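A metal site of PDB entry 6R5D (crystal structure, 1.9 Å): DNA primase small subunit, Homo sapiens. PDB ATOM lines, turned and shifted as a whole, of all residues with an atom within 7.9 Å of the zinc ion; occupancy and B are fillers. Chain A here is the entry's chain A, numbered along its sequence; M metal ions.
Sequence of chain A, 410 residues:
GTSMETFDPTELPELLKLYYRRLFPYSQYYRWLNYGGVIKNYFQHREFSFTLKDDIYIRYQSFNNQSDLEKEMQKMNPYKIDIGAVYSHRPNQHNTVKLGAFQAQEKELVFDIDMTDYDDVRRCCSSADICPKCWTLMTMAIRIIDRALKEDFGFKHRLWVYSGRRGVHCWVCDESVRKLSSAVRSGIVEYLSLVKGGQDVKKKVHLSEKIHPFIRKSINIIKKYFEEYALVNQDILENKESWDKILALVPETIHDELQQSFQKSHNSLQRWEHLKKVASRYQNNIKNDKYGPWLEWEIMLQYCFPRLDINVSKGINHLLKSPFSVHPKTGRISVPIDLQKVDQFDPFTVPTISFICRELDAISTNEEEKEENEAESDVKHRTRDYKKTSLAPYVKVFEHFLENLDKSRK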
ATOM      1  N   MET A 115      17.113  -0.326   2.144  1.00  0.00           N
ATOM      2  CA  MET A 115      16.099  -0.968   1.312  1.00  0.00           C
ATOM      3  C   MET A 115      16.368  -2.460   1.146  1.00  0.00           C
ATOM      4  O   MET A 115      15.436  -3.250   0.983  1.00  0.00           O
ATOM      5  CB  MET A 115      16.033  -0.299  -0.057  1.00  0.00           C
ATOM      6  CG  MET A 115      14.702  -0.470  -0.767  1.00  0.00           C
ATOM      7  SD  MET A 115      13.518   0.787  -0.251  1.00  0.00           S
ATOM      8  CE  MET A 115      14.246   2.224  -1.031  1.00  0.00           C
ATOM      9  N   ARG A 122       9.914  -7.011  -1.499  1.00  0.00           N
ATOM     10  CA  ARG A 122      10.096  -6.241  -2.714  1.00  0.00           C
ATOM     11  C   ARG A 122      10.090  -7.190  -3.912  1.00  0.00           C
ATOM     12  O   ARG A 122      10.790  -8.204  -3.890  1.00  0.00           O
ATOM     13  CB  ARG A 122      11.423  -5.470  -2.726  1.00  0.00           C
ATOM     14  CG  ARG A 122      11.495  -4.230  -1.892  1.00  0.00           C
ATOM     15  CD  ARG A 122      12.633  -3.331  -2.402  1.00  0.00           C
ATOM     16  NE  ARG A 122      13.958  -3.937  -2.300  1.00  0.00           N
ATOM     17  CZ  ARG A 122      15.075  -3.359  -2.760  1.00  0.00           C
ATOM     18  NH1 ARG A 122      15.015  -2.183  -3.356  1.00  0.00           N
ATOM     19  NH2 ARG A 122      16.254  -3.957  -2.624  1.00  0.00           N
ATOM     20  N   ARG A 123       9.336  -6.839  -4.953  1.00  0.00           N
ATOM     21  CA  ARG A 123       9.368  -7.611  -6.202  1.00  0.00           C
ATOM     22  C   ARG A 123      10.183  -6.939  -7.297  1.00  0.00           C
ATOM     23  O   ARG A 123      10.679  -7.641  -8.192  1.00  0.00           O
ATOM     24  CB  ARG A 123       7.943  -7.835  -6.729  1.00  0.00           C
ATOM     25  CG  ARG A 123       7.084  -8.724  -5.853  1.00  0.00           C
ATOM     26  CD  ARG A 123       5.716  -8.931  -6.487  1.00  0.00           C
ATOM     27  NE  ARG A 123       5.792  -9.705  -7.722  1.00  0.00           N
ATOM     28  CZ  ARG A 123       4.859  -9.703  -8.670  1.00  0.00           C
ATOM     29  NH1 ARG A 123       3.770  -8.957  -8.553  1.00  0.00           N
ATOM     30  NH2 ARG A 123       5.019 -10.450  -9.765  1.00  0.00           N
ATOM     31  N   CYS A 124      10.336  -5.618  -7.261  1.00  0.00           N
ATOM     32  CA  CYS A 124      10.949  -4.887  -8.363  1.00  0.00           C
ATOM     33  C   CYS A 124      12.466  -4.944  -8.332  1.00  0.00           C
ATOM     34  O   CYS A 124      13.099  -5.078  -9.378  1.00  0.00           O
ATOM     35  CB  CYS A 124      10.476  -3.432  -8.312  1.00  0.00           C
ATOM     36  SG  CYS A 124      10.585  -2.740  -6.648  1.00  0.00           S
ATOM     37  N   CYS A 125      13.075  -4.848  -7.139  1.00  0.00           N
ATOM     38  CA  CYS A 125      14.517  -4.703  -6.998  1.00  0.00           C
ATOM     39  C   CYS A 125      15.051  -5.691  -5.964  1.00  0.00           C
ATOM     40  O   CYS A 125      14.292  -6.258  -5.169  1.00  0.00           O
ATOM     41  CB  CYS A 125      14.900  -3.283  -6.547  1.00  0.00           C
ATOM     42  SG  CYS A 125      14.405  -1.925  -7.626  1.00  0.00           S
ATOM     43  N   SER A 126      16.370  -5.866  -5.975  1.00  0.00           N
ATOM     44  CA  SER A 126      17.044  -6.683  -4.982  1.00  0.00           C
ATOM     45  C   SER A 126      18.426  -6.094  -4.705  1.00  0.00           C
ATOM     46  O   SER A 126      18.951  -5.306  -5.489  1.00  0.00           O
ATOM     47  CB  SER A 126      17.177  -8.143  -5.437  1.00  0.00           C
ATOM     48  OG  SER A 126      18.053  -8.252  -6.541  1.00  0.00           O
ATOM     49  N   ASP A 129      19.895  -2.263  -5.305  1.00  0.00           N
ATOM     50  CA  ASP A 129      19.087  -1.537  -6.276  1.00  0.00           C
ATOM     51  C   ASP A 129      17.870  -0.914  -5.616  1.00  0.00           C
ATOM     52  O   ASP A 129      17.326  -1.443  -4.640  1.00  0.00           O
ATOM     53  CB  ASP A 129      18.626  -2.478  -7.394  1.00  0.00           C
ATOM     54  CG  ASP A 129      19.763  -2.879  -8.328  1.00  0.00           C
ATOM     55  OD1 ASP A 129      20.699  -2.068  -8.525  1.00  0.00           O
ATOM     56  OD2 ASP A 129      19.719  -4.001  -8.872  1.00  0.00           O
ATOM     57  N   ILE A 130      17.439   0.227  -6.151  1.00  0.00           N
ATOM     58  CA  ILE A 130      16.199   0.878  -5.763  1.00  0.00           C
ATOM     59  C   ILE A 130      15.544   1.430  -7.026  1.00  0.00           C
ATOM     60  O   ILE A 130      16.195   1.635  -8.054  1.00  0.00           O
ATOM     61  CB  ILE A 130      16.406   2.013  -4.742  1.00  0.00           C
ATOM     62  CG1 ILE A 130      17.358   3.080  -5.294  1.00  0.00           C
ATOM     63  CG2 ILE A 130      16.940   1.436  -3.437  1.00  0.00           C
ATOM     64  CD1 ILE A 130      17.469   4.320  -4.418  1.00  0.00           C
ATOM     65  N   CYS A 131      14.244   1.658  -6.944  1.00  0.00           N
ATOM     66  CA  CYS A 131      13.498   2.247  -8.053  1.00  0.00           C
ATOM     67  C   CYS A 131      12.293   2.957  -7.477  1.00  0.00           C
ATOM     68  O   CYS A 131      11.970   2.810  -6.288  1.00  0.00           O
ATOM     69  CB  CYS A 131      13.071   1.183  -9.070  1.00  0.00           C
ATOM     70  SG  CYS A 131      11.598   0.252  -8.603  1.00  0.00           S
ATOM     71  N   PRO A 132      11.590   3.747  -8.293  1.00  0.00           N
ATOM     72  CA  PRO A 132      10.421   4.477  -7.777  1.00  0.00           C
ATOM     73  C   PRO A 132       9.306   3.572  -7.285  1.00  0.00           C
ATOM     74  O   PRO A 132       8.444   4.030  -6.521  1.00  0.00           O
ATOM     75  CB  PRO A 132       9.971   5.317  -8.974  1.00  0.00           C
ATOM     76  CG  PRO A 132      11.189   5.423  -9.855  1.00  0.00           C
ATOM     77  CD  PRO A 132      11.879   4.095  -9.696  1.00  0.00           C
ATOM     78  N   LYS A 133       9.272   2.300  -7.694  1.00  0.00           N
ATOM     79  CA  LYS A 133       8.202   1.401  -7.281  1.00  0.00           C
ATOM     80  C   LYS A 133       8.403   0.863  -5.873  1.00  0.00           C
ATOM     81  O   LYS A 133       7.430   0.368  -5.275  1.00  0.00           O
ATOM     82  CB  LYS A 133       8.078   0.238  -8.265  1.00  0.00           C
ATOM     83  CG  LYS A 133       7.906   0.658  -9.716  1.00  0.00           C
ATOM     84  CD  LYS A 133       7.828  -0.534 -10.663  1.00  0.00           C
ATOM     85  CE  LYS A 133       6.502  -1.283 -10.531  1.00  0.00           C
ATOM     86  NZ  LYS A 133       5.327  -0.416 -10.859  1.00  0.00           N
ATOM     87  N   CYS A 134       9.617   0.927  -5.331  1.00  0.00           N
ATOM     88  CA  CYS A 134       9.883   0.517  -3.966  1.00  0.00           C
ATOM     89  C   CYS A 134      10.370   1.637  -3.066  1.00  0.00           C
ATOM     90  O   CYS A 134      10.469   1.426  -1.850  1.00  0.00           O
ATOM     91  CB  CYS A 134      10.898  -0.637  -3.920  1.00  0.00           C
ATOM     92  SG  CYS A 134      12.532  -0.327  -4.681  1.00  0.00           S
ATOM     93  N   TRP A 135      10.680   2.831  -3.605  1.00  0.00           N
ATOM     94  CA  TRP A 135      11.116   3.917  -2.739  1.00  0.00           C
ATOM     95  C   TRP A 135      10.039   4.338  -1.747  1.00  0.00           C
ATOM     96  O   TRP A 135      10.360   4.884  -0.692  1.00  0.00           O
ATOM     97  CB  TRP A 135      11.550   5.139  -3.563  1.00  0.00           C
ATOM     98  CG  TRP A 135      12.072   6.204  -2.653  1.00  0.00           C
ATOM     99  CD1 TRP A 135      11.439   7.343  -2.265  1.00  0.00           C
ATOM    100  CD2 TRP A 135      13.333   6.194  -1.990  1.00  0.00           C
ATOM    101  NE1 TRP A 135      12.237   8.053  -1.399  1.00  0.00           N
ATOM    102  CE2 TRP A 135      13.413   7.372  -1.214  1.00  0.00           C
ATOM    103  CE3 TRP A 135      14.415   5.308  -1.976  1.00  0.00           C
ATOM    104  CZ2 TRP A 135      14.515   7.676  -0.442  1.00  0.00           C
ATOM    105  CZ3 TRP A 135      15.509   5.617  -1.205  1.00  0.00           C
ATOM    106  CH2 TRP A 135      15.554   6.792  -0.443  1.00  0.00           C
ATOM    107  N   LEU A 137       8.655   2.645   0.279  1.00  0.00           N
ATOM    108  CA  LEU A 137       8.973   2.045   1.573  1.00  0.00           C
ATOM    109  C   LEU A 137       9.714   3.032   2.459  1.00  0.00           C
ATOM    110  O   LEU A 137       9.469   3.094   3.679  1.00  0.00           O
ATOM    111  CB  LEU A 137       9.814   0.780   1.364  1.00  0.00           C
ATOM    112  CG  LEU A 137       9.069  -0.436   0.790  1.00  0.00           C
ATOM    113  CD1 LEU A 137      10.045  -1.549   0.446  1.00  0.00           C
ATOM    114  CD2 LEU A 137       8.017  -0.932   1.770  1.00  0.00           C
ATOM    115  N   TYR A 229       0.990   1.508  -3.349  1.00  0.00           N
ATOM    116  CA  TYR A 229       2.296   0.863  -3.218  1.00  0.00           C
ATOM    117  C   TYR A 229       2.185  -0.650  -3.406  1.00  0.00           C
ATOM    118  O   TYR A 229       2.807  -1.229  -4.305  1.00  0.00           O
ATOM    119  CB  TYR A 229       2.940   1.159  -1.871  1.00  0.00           C
ATOM    120  CG  TYR A 229       4.127   0.253  -1.667  1.00  0.00           C
ATOM    121  CD1 TYR A 229       5.264   0.392  -2.463  1.00  0.00           C
ATOM    122  CD2 TYR A 229       4.093  -0.778  -0.746  1.00  0.00           C
ATOM    123  CE1 TYR A 229       6.336  -0.449  -2.318  1.00  0.00           C
ATOM    124  CE2 TYR A 229       5.181  -1.629  -0.597  1.00  0.00           C
ATOM    125  CZ  TYR A 229       6.290  -1.457  -1.386  1.00  0.00           C
ATOM    126  OH  TYR A 229       7.369  -2.293  -1.261  1.00  0.00           O
ATOM    127  N   GLN A 234       3.573  -2.909  -6.489  1.00  0.00           N
ATOM    128  CA  GLN A 234       4.146  -4.216  -6.220  1.00  0.00           C
ATOM    129  C   GLN A 234       3.227  -5.359  -6.655  1.00  0.00           C
ATOM    130  O   GLN A 234       3.717  -6.470  -6.902  1.00  0.00           O
ATOM    131  CB  GLN A 234       4.473  -4.375  -4.729  1.00  0.00           C
ATOM    132  CG  GLN A 234       5.555  -3.427  -4.218  1.00  0.00           C
ATOM    133  CD  GLN A 234       6.894  -3.634  -4.898  1.00  0.00           C
ATOM    134  OE1 GLN A 234       7.356  -4.763  -5.062  1.00  0.00           O
ATOM    135  NE2 GLN A 234       7.527  -2.529  -5.295  1.00  0.00           N
ATOM    136  N   PHE A 348      16.658   9.731  -7.661  1.00  0.00           N
ATOM    137  CA  PHE A 348      17.354   9.772  -8.948  1.00  0.00           C
ATOM    138  C   PHE A 348      17.572  11.181  -9.483  1.00  0.00           C
ATOM    139  O   PHE A 348      18.296  11.348 -10.460  1.00  0.00           O
ATOM    140  CB  PHE A 348      16.575   8.928  -9.965  1.00  0.00           C
ATOM    141  CG  PHE A 348      16.599   7.471  -9.648  1.00  0.00           C
ATOM    142  CD1 PHE A 348      17.646   6.674 -10.070  1.00  0.00           C
ATOM    143  CD2 PHE A 348      15.604   6.903  -8.876  1.00  0.00           C
ATOM    144  CE1 PHE A 348      17.685   5.334  -9.752  1.00  0.00           C
ATOM    145  CE2 PHE A 348      15.629   5.562  -8.553  1.00  0.00           C
ATOM    146  CZ  PHE A 348      16.675   4.775  -8.997  1.00  0.00           C
HETATM  147 ZN    ZN M   1      12.290  -1.267  -6.871  1.00  0.00          ZN
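Four residues have an atom within 4 Å of the zinc ion: Cys 124, Cys 125, Cys 131 and Cys 134. Along chain A the residues within 4 Å of the zinc ion span positions 124 to 134.
The zinc ion is bound by the side-chain sulfur of Cys 124 (2.3 Å), the side-chain sulfur of Cys 125 (2.3 Å), the side-chain sulfur of Cys 134 (2.4 Å) and the side-chain sulfur of Cys 131 (2.4 Å).
The backbone NH (N) of Lys 133 sits close to the side-chain sulfur (SG) of Cys 131 (3.2 Å). The side-chain sulfur (SG) of Cys 124 sits close to the side-chain amide nitrogen (NE2) of Gln 234 (3.4 Å). SG of Cys 134 sits close to NH1 of Arg 122 (3.4 Å).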
